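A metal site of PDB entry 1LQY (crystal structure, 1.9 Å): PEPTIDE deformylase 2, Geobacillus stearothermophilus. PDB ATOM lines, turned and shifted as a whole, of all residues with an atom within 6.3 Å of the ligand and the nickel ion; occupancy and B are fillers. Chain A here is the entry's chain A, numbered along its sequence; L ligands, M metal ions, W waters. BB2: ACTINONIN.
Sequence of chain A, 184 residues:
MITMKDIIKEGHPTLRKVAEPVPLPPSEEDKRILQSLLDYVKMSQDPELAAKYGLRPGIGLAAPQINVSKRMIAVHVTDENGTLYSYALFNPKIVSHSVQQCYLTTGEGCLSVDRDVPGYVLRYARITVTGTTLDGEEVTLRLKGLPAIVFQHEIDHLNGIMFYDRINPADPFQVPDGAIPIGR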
ATOM      1  N   PRO A  57     -24.477   3.082   7.006  1.00  0.00           N
ATOM      2  CA  PRO A  57     -23.420   3.378   7.976  1.00  0.00           C
ATOM      3  C   PRO A  57     -23.875   3.919   9.325  1.00  0.00           C
ATOM      4  O   PRO A  57     -24.620   4.902   9.412  1.00  0.00           O
ATOM      5  CB  PRO A  57     -22.485   4.353   7.230  1.00  0.00           C
ATOM      6  CG  PRO A  57     -23.248   4.852   6.077  1.00  0.00           C
ATOM      7  CD  PRO A  57     -24.342   3.860   5.763  1.00  0.00           C
ATOM      8  N   GLY A  58     -23.425   3.249  10.373  1.00  0.00           N
ATOM      9  CA  GLY A  58     -23.743   3.690  11.716  1.00  0.00           C
ATOM     10  C   GLY A  58     -22.472   3.596  12.539  1.00  0.00           C
ATOM     11  O   GLY A  58     -21.679   2.657  12.355  1.00  0.00           O
ATOM     12  N   ILE A  59     -22.251   4.550  13.444  1.00  0.00           N
ATOM     13  CA  ILE A  59     -21.071   4.494  14.280  1.00  0.00           C
ATOM     14  C   ILE A  59     -21.411   3.913  15.659  1.00  0.00           C
ATOM     15  O   ILE A  59     -20.573   3.849  16.558  1.00  0.00           O
ATOM     16  CB  ILE A  59     -20.437   5.892  14.425  1.00  0.00           C
ATOM     17  CG1 ILE A  59     -21.468   6.916  14.898  1.00  0.00           C
ATOM     18  CG2 ILE A  59     -19.909   6.328  13.087  1.00  0.00           C
ATOM     19  CD1 ILE A  59     -20.872   8.316  15.087  1.00  0.00           C
ATOM     20  N   GLY A  60     -22.669   3.493  15.799  1.00  0.00           N
ATOM     21  CA  GLY A  60     -23.102   2.853  17.041  1.00  0.00           C
ATOM     22  C   GLY A  60     -24.401   2.098  16.798  1.00  0.00           C
ATOM     23  O   GLY A  60     -25.122   2.382  15.845  1.00  0.00           O
ATOM     24  N   LEU A  61     -24.720   1.107  17.629  1.00  0.00           N
ATOM     25  CA  LEU A  61     -25.991   0.407  17.449  1.00  0.00           C
ATOM     26  C   LEU A  61     -26.469  -0.203  18.778  1.00  0.00           C
ATOM     27  O   LEU A  61     -25.658  -0.617  19.588  1.00  0.00           O
ATOM     28  CB  LEU A  61     -25.858  -0.710  16.403  1.00  0.00           C
ATOM     29  CG  LEU A  61     -27.201  -1.321  15.992  1.00  0.00           C
ATOM     30  CD1 LEU A  61     -27.980  -0.388  15.092  1.00  0.00           C
ATOM     31  CD2 LEU A  61     -26.921  -2.652  15.312  1.00  0.00           C
ATOM     32  N   ALA A  62     -27.792  -0.256  18.972  1.00  0.00           N
ATOM     33  CA  ALA A  62     -28.332  -0.844  20.226  1.00  0.00           C
ATOM     34  C   ALA A  62     -29.309  -2.018  19.938  1.00  0.00           C
ATOM     35  O   ALA A  62     -30.017  -2.001  18.951  1.00  0.00           O
ATOM     36  CB  ALA A  62     -29.014   0.243  21.046  1.00  0.00           C
ATOM     37  N   GLN A  65     -32.820  -1.787  18.329  1.00  0.00           N
ATOM     38  CA  GLN A  65     -32.991  -1.384  16.916  1.00  0.00           C
ATOM     39  C   GLN A  65     -33.226  -2.582  15.981  1.00  0.00           C
ATOM     40  O   GLN A  65     -33.741  -2.408  14.877  1.00  0.00           O
ATOM     41  CB  GLN A  65     -31.806  -0.533  16.424  1.00  0.00           C
ATOM     42  CG  GLN A  65     -31.780   0.831  17.087  1.00  0.00           C
ATOM     43  CD  GLN A  65     -30.538   1.618  16.765  1.00  0.00           C
ATOM     44  OE1 GLN A  65     -29.447   1.360  17.291  1.00  0.00           O
ATOM     45  NE2 GLN A  65     -30.694   2.579  15.876  1.00  0.00           N
ATOM     46  N   LEU A 104     -23.530  18.147  18.167  1.00  0.00           N
ATOM     47  CA  LEU A 104     -23.005  18.170  16.788  1.00  0.00           C
ATOM     48  C   LEU A 104     -23.755  19.282  16.043  1.00  0.00           C
ATOM     49  O   LEU A 104     -24.981  19.353  16.085  1.00  0.00           O
ATOM     50  CB  LEU A 104     -23.309  16.820  16.106  1.00  0.00           C
ATOM     51  CG  LEU A 104     -22.255  15.721  16.048  1.00  0.00           C
ATOM     52  CD1 LEU A 104     -21.251  15.833  17.120  1.00  0.00           C
ATOM     53  CD2 LEU A 104     -22.957  14.383  16.106  1.00  0.00           C
ATOM     54  N   THR A 106     -24.316  19.542  13.002  1.00  0.00           N
ATOM     55  CA  THR A 106     -25.118  18.949  11.923  1.00  0.00           C
ATOM     56  C   THR A 106     -26.391  18.295  12.448  1.00  0.00           C
ATOM     57  O   THR A 106     -27.275  17.935  11.659  1.00  0.00           O
ATOM     58  CB  THR A 106     -24.384  17.793  11.229  1.00  0.00           C
ATOM     59  OG1 THR A 106     -24.111  16.779  12.199  1.00  0.00           O
ATOM     60  CG2 THR A 106     -23.102  18.267  10.572  1.00  0.00           C
ATOM     61  N   GLY A 107     -26.487  18.130  13.766  1.00  0.00           N
ATOM     62  CA  GLY A 107     -27.630  17.416  14.323  1.00  0.00           C
ATOM     63  C   GLY A 107     -27.240  15.936  14.231  1.00  0.00           C
ATOM     64  O   GLY A 107     -26.097  15.615  13.859  1.00  0.00           O
ATOM     65  N   GLU A 108     -28.148  15.042  14.597  1.00  0.00           N
ATOM     66  CA  GLU A 108     -27.863  13.624  14.572  1.00  0.00           C
ATOM     67  C   GLU A 108     -28.865  12.888  13.658  1.00  0.00           C
ATOM     68  O   GLU A 108     -29.995  13.356  13.411  1.00  0.00           O
ATOM     69  CB  GLU A 108     -27.950  13.014  15.993  1.00  0.00           C
ATOM     70  CG  GLU A 108     -26.966  13.615  17.008  1.00  0.00           C
ATOM     71  CD  GLU A 108     -27.089  13.018  18.412  1.00  0.00           C
ATOM     72  OE1 GLU A 108     -27.846  12.016  18.609  1.00  0.00           O
ATOM     73  OE2 GLU A 108     -26.407  13.532  19.332  1.00  0.00           O
ATOM     74  N   GLY A 109     -28.431  11.734  13.171  1.00  0.00           N
ATOM     75  CA  GLY A 109     -29.305  10.914  12.354  1.00  0.00           C
ATOM     76  C   GLY A 109     -29.436   9.595  13.106  1.00  0.00           C
ATOM     77  O   GLY A 109     -28.575   9.262  13.928  1.00  0.00           O
ATOM     78  N   CYS A 110     -30.508   8.855  12.820  1.00  0.00           N
ATOM     79  CA  CYS A 110     -30.747   7.580  13.486  1.00  0.00           C
ATOM     80  C   CYS A 110     -31.111   6.541  12.429  1.00  0.00           C
ATOM     81  O   CYS A 110     -31.875   6.815  11.514  1.00  0.00           O
ATOM     82  CB  CYS A 110     -31.921   7.699  14.508  1.00  0.00           C
ATOM     83  SG  CYS A 110     -32.134   6.261  15.618  1.00  0.00           S
ATOM     84  N   LEU A 111     -30.560   5.358  12.569  1.00  0.00           N
ATOM     85  CA  LEU A 111     -30.849   4.299  11.589  1.00  0.00           C
ATOM     86  C   LEU A 111     -32.346   3.974  11.559  1.00  0.00           C
ATOM     87  O   LEU A 111     -32.866   3.579  10.530  1.00  0.00           O
ATOM     88  CB  LEU A 111     -30.015   3.061  11.938  1.00  0.00           C
ATOM     89  CG  LEU A 111     -28.751   2.771  11.133  1.00  0.00           C
ATOM     90  CD1 LEU A 111     -28.065   4.036  10.727  1.00  0.00           C
ATOM     91  CD2 LEU A 111     -27.809   1.894  11.941  1.00  0.00           C
ATOM     92  N   SER A 112     -33.054   4.141  12.696  1.00  0.00           N
ATOM     93  CA  SER A 112     -34.496   3.848  12.725  1.00  0.00           C
ATOM     94  C   SER A 112     -35.388   5.036  12.279  1.00  0.00           C
ATOM     95  O   SER A 112     -36.622   4.890  12.200  1.00  0.00           O
ATOM     96  CB  SER A 112     -34.914   3.405  14.143  1.00  0.00           C
ATOM     97  OG  SER A 112     -34.029   2.443  14.701  1.00  0.00           O
ATOM     98  N   ARG A 123     -26.162  17.110  24.476  1.00  0.00           N
ATOM     99  CA  ARG A 123     -25.535  15.975  25.127  1.00  0.00           C
ATOM    100  C   ARG A 123     -24.542  16.455  26.166  1.00  0.00           C
ATOM    101  O   ARG A 123     -24.102  17.606  26.126  1.00  0.00           O
ATOM    102  CB  ARG A 123     -24.768  15.139  24.094  1.00  0.00           C
ATOM    103  CG  ARG A 123     -25.589  14.699  22.860  1.00  0.00           C
ATOM    104  CD  ARG A 123     -26.246  13.362  23.159  1.00  0.00           C
ATOM    105  NE  ARG A 123     -26.971  12.737  22.049  1.00  0.00           N
ATOM    106  CZ  ARG A 123     -27.959  11.855  22.226  1.00  0.00           C
ATOM    107  NH1 ARG A 123     -28.324  11.525  23.461  1.00  0.00           N
ATOM    108  NH2 ARG A 123     -28.595  11.304  21.188  1.00  0.00           N
ATOM    109  N   LEU A 146     -17.336  13.362  20.597  1.00  0.00           N
ATOM    110  CA  LEU A 146     -18.115  12.447  19.761  1.00  0.00           C
ATOM    111  C   LEU A 146     -18.250  11.064  20.380  1.00  0.00           C
ATOM    112  O   LEU A 146     -19.328  10.482  20.328  1.00  0.00           O
ATOM    113  CB  LEU A 146     -17.538  12.343  18.352  1.00  0.00           C
ATOM    114  CG  LEU A 146     -18.323  11.412  17.419  1.00  0.00           C
ATOM    115  CD1 LEU A 146     -19.748  11.915  17.184  1.00  0.00           C
ATOM    116  CD2 LEU A 146     -17.587  11.363  16.078  1.00  0.00           C
ATOM    117  N   ILE A 149     -20.940  11.257  22.937  1.00  0.00           N
ATOM    118  CA  ILE A 149     -22.222  11.451  22.292  1.00  0.00           C
ATOM    119  C   ILE A 149     -22.756  10.117  21.785  1.00  0.00           C
ATOM    120  O   ILE A 149     -23.939   9.818  21.983  1.00  0.00           O
ATOM    121  CB  ILE A 149     -22.083  12.460  21.105  1.00  0.00           C
ATOM    122  CG1 ILE A 149     -21.786  13.857  21.673  1.00  0.00           C
ATOM    123  CG2 ILE A 149     -23.391  12.571  20.342  1.00  0.00           C
ATOM    124  CD1 ILE A 149     -21.790  14.946  20.611  1.00  0.00           C
ATOM    125  N   VAL A 150     -21.904   9.317  21.124  1.00  0.00           N
ATOM    126  CA  VAL A 150     -22.371   8.030  20.604  1.00  0.00           C
ATOM    127  C   VAL A 150     -22.856   7.121  21.736  1.00  0.00           C
ATOM    128  O   VAL A 150     -23.912   6.495  21.620  1.00  0.00           O
ATOM    129  CB  VAL A 150     -21.253   7.279  19.783  1.00  0.00           C
ATOM    130  CG1 VAL A 150     -21.852   6.027  19.163  1.00  0.00           C
ATOM    131  CG2 VAL A 150     -20.701   8.185  18.649  1.00  0.00           C
ATOM    132  N   HIS A 153     -26.237   8.308  22.846  1.00  0.00           N
ATOM    133  CA  HIS A 153     -27.261   7.968  21.860  1.00  0.00           C
ATOM    134  C   HIS A 153     -27.681   6.475  21.969  1.00  0.00           C
ATOM    135  O   HIS A 153     -28.875   6.160  21.989  1.00  0.00           O
ATOM    136  CB  HIS A 153     -26.692   8.236  20.440  1.00  0.00           C
ATOM    137  CG  HIS A 153     -27.666   7.921  19.332  1.00  0.00           C
ATOM    138  ND1 HIS A 153     -28.237   8.904  18.550  1.00  0.00           N
ATOM    139  CD2 HIS A 153     -28.125   6.742  18.856  1.00  0.00           C
ATOM    140  CE1 HIS A 153     -29.016   8.342  17.645  1.00  0.00           C
ATOM    141  NE2 HIS A 153     -28.967   7.026  17.812  1.00  0.00           N
ATOM    142  N   GLU A 154     -26.723   5.576  22.053  1.00  0.00           N
ATOM    143  CA  GLU A 154     -27.052   4.145  22.127  1.00  0.00           C
ATOM    144  C   GLU A 154     -27.654   3.801  23.492  1.00  0.00           C
ATOM    145  O   GLU A 154     -28.594   3.021  23.593  1.00  0.00           O
ATOM    146  CB  GLU A 154     -25.822   3.244  21.894  1.00  0.00           C
ATOM    147  CG  GLU A 154     -25.038   3.473  20.567  1.00  0.00           C
ATOM    148  CD  GLU A 154     -25.935   3.688  19.355  1.00  0.00           C
ATOM    149  OE1 GLU A 154     -27.061   3.116  19.284  1.00  0.00           O
ATOM    150  OE2 GLU A 154     -25.518   4.438  18.446  1.00  0.00           O
ATOM    151  N   HIS A 157     -31.330   4.605  23.575  1.00  0.00           N
ATOM    152  CA  HIS A 157     -32.205   3.595  22.970  1.00  0.00           C
ATOM    153  C   HIS A 157     -32.644   2.544  23.976  1.00  0.00           C
ATOM    154  O   HIS A 157     -33.774   2.060  23.875  1.00  0.00           O
ATOM    155  CB  HIS A 157     -31.526   2.836  21.831  1.00  0.00           C
ATOM    156  CG  HIS A 157     -31.500   3.578  20.549  1.00  0.00           C
ATOM    157  ND1 HIS A 157     -32.644   4.075  19.956  1.00  0.00           N
ATOM    158  CD2 HIS A 157     -30.472   3.909  19.723  1.00  0.00           C
ATOM    159  CE1 HIS A 157     -32.316   4.679  18.824  1.00  0.00           C
ATOM    160  NE2 HIS A 157     -31.004   4.593  18.668  1.00  0.00           N
ATOM    161  N   PHE A 163     -33.294  10.375  19.836  1.00  0.00           N
ATOM    162  CA  PHE A 163     -32.509  11.609  19.792  1.00  0.00           C
ATOM    163  C   PHE A 163     -33.328  12.882  19.726  1.00  0.00           C
ATOM    164  O   PHE A 163     -33.005  13.861  20.401  1.00  0.00           O
ATOM    165  CB  PHE A 163     -31.499  11.543  18.629  1.00  0.00           C
ATOM    166  CG  PHE A 163     -32.114  11.797  17.267  1.00  0.00           C
ATOM    167  CD1 PHE A 163     -32.196  13.091  16.749  1.00  0.00           C
ATOM    168  CD2 PHE A 163     -32.551  10.729  16.475  1.00  0.00           C
ATOM    169  CE1 PHE A 163     -32.691  13.339  15.447  1.00  0.00           C
ATOM    170  CE2 PHE A 163     -33.042  10.960  15.171  1.00  0.00           C
ATOM    171  CZ  PHE A 163     -33.107  12.268  14.663  1.00  0.00           C
HETATM  172  C5  BB2 L   1     -26.605   5.196  14.241  1.00  0.00           C
HETATM  173  C3  BB2 L   1     -27.753   4.825  15.220  1.00  0.00           C
HETATM  174  O4  BB2 L   1     -28.924   5.129  14.968  1.00  0.00           O
HETATM  175  N1  BB2 L   1     -27.454   4.176  16.340  1.00  0.00           N
HETATM  176  O2  BB2 L   1     -28.487   3.837  17.235  1.00  0.00           O
HETATM  177  C6  BB2 L   1     -26.162   6.616  14.615  1.00  0.00           C
HETATM  178  C12 BB2 L   1     -25.353   7.221  13.431  1.00  0.00           C
HETATM  179  O13 BB2 L   1     -24.367   6.600  12.955  1.00  0.00           O
HETATM  180  C7  BB2 L   1     -25.278   6.533  15.910  1.00  0.00           C
HETATM  181  C8  BB2 L   1     -24.523   7.833  16.304  1.00  0.00           C
HETATM  182  C9  BB2 L   1     -25.490   8.936  16.716  1.00  0.00           C
HETATM  183  C10 BB2 L   1     -24.718  10.039  17.487  1.00  0.00           C
HETATM  184  C11 BB2 L   1     -23.903  11.008  16.618  1.00  0.00           C
HETATM  185  N14 BB2 L   1     -25.836   8.478  13.039  1.00  0.00           N
HETATM  186  C15 BB2 L   1     -25.125   9.084  11.974  1.00  0.00           C
HETATM  187  C16 BB2 L   1     -26.041   9.311  10.740  1.00  0.00           C
HETATM  188  C18 BB2 L   1     -25.330  10.129   9.624  1.00  0.00           C
HETATM  189  C17 BB2 L   1     -26.508   7.961  10.169  1.00  0.00           C
HETATM  190  C19 BB2 L   1     -24.651  10.473  12.507  1.00  0.00           C
HETATM  191  O20 BB2 L   1     -25.514  11.153  13.117  1.00  0.00           O
HETATM  192  N21 BB2 L   1     -23.421  10.991  12.166  1.00  0.00           N
HETATM  193  C22 BB2 L   1     -22.923  12.191  12.894  1.00  0.00           C
HETATM  194  C23 BB2 L   1     -22.330   9.994  12.118  1.00  0.00           C
HETATM  195  C24 BB2 L   1     -21.055  10.867  12.199  1.00  0.00           C
HETATM  196  C25 BB2 L   1     -21.457  11.902  13.238  1.00  0.00           C
HETATM  197  C26 BB2 L   1     -23.180  13.316  11.890  1.00  0.00           C
HETATM  198  O27 BB2 L   1     -23.202  14.458  12.310  1.00  0.00           O
HETATM  199 NI    NI M   1     -29.964   5.363  16.931  1.00  0.00          NI
HETATM  200  O   HOH W   1     -28.563  10.936   9.087  1.00  0.00           O
HETATM  201  O   HOH W   2     -20.447  15.872  12.942  1.00  0.00           O
HETATM  202  O   HOH W   3     -22.938   6.823  10.263  1.00  0.00           O
HETATM  203  O   HOH W   4     -26.649   5.827   7.538  1.00  0.00           O
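The nickel ion is bound by a ring nitrogen (NE2) of His 153 (2.1 Å), an oxygen (O2) of the ligand (2.1 Å), a ring nitrogen (NE2) of His 157 (2.2 Å), an oxygen (O4) of the ligand (2.2 Å) and the side-chain sulfur (SG) of Cys 110 (2.7 Å).
Water W3 lies within hydrogen-bond range of the backbone carbonyl oxygen (O) of Pro 57 (2.7 Å) and an oxygen (O13) of the ligand (3.1 Å).
Merely in contact with the ligand: Pro 57, Gly 58, Leu 104 and Glu 108.
Hydrophobic or aromatic side chains within 4 Å of the ligand: Ile 59, Leu 104, Leu 111, His 153 and His 157.
Of the 23 residues printed, 15 come within 4 Å of the ligand.
An oxygen (O27) of the ligand sits at hydrogen-bond distance from the side-chain hydroxyl (OG1) of Thr 106 (2.5 Å).
OE2 of Glu 154 is in hydrogen-bond range of N1 of the ligand (2.9 Å).
An oxygen (O2) of the ligand lies close to the side-chain amide oxygen of Gln 65, 2.7 Å away.
An oxygen (O4) of the ligand lies close to the backbone NH of Leu 111 (2.9 Å).
An oxygen (O20) of the ligand lies within hydrogen-bond range of the backbone NH of Gly 109 (3.0 Å).
N14 of the ligand is in hydrogen-bond range of O of Gly 109 (3.0 Å).
The backbone carbonyl oxygen of Gly 60 lies within hydrogen-bond range of a nitrogen (N1) of the ligand (3.0 Å).
An oxygen (O13) of the ligand sits at hydrogen-bond distance from the backbone NH (N) of Ile 59, 3.0 Å away.
An oxygen (O27) of the ligand is in hydrogen-bond range of the backbone carbonyl oxygen of Gly 107, 3.5 Å away.
Merely in contact with the nickel ion: Gln 65.
Of the 23 residues printed, 4 come within 4 Å of the nickel ion.
A ring nitrogen (ND1) of His 153 is in hydrogen-bond range of the side-chain carboxylate (OE1) of Glu 108 (3.1 Å).
A ring nitrogen (NE2) of His 157 sits close to the side-chain amide nitrogen (NE2) of Gln 65, 3.5 Å away.
The side-chain carboxylate (OE1) of Glu 154 sits at hydrogen-bond distance from the backbone NH (N) of Ala 62, 3.5 Å away.
The backbone NH (N) of Ala 62 lies within hydrogen-bond range of the side-chain amide oxygen (OE1) of Gln 65, at 2.9 Å.
N of Ser 112 lies close to SG of Cys 110, at 3.7 Å.
The guanidinium group of Arg 123 lies within salt-bridge range of the side-chain carboxylate of Glu 108 (2.8 Å).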
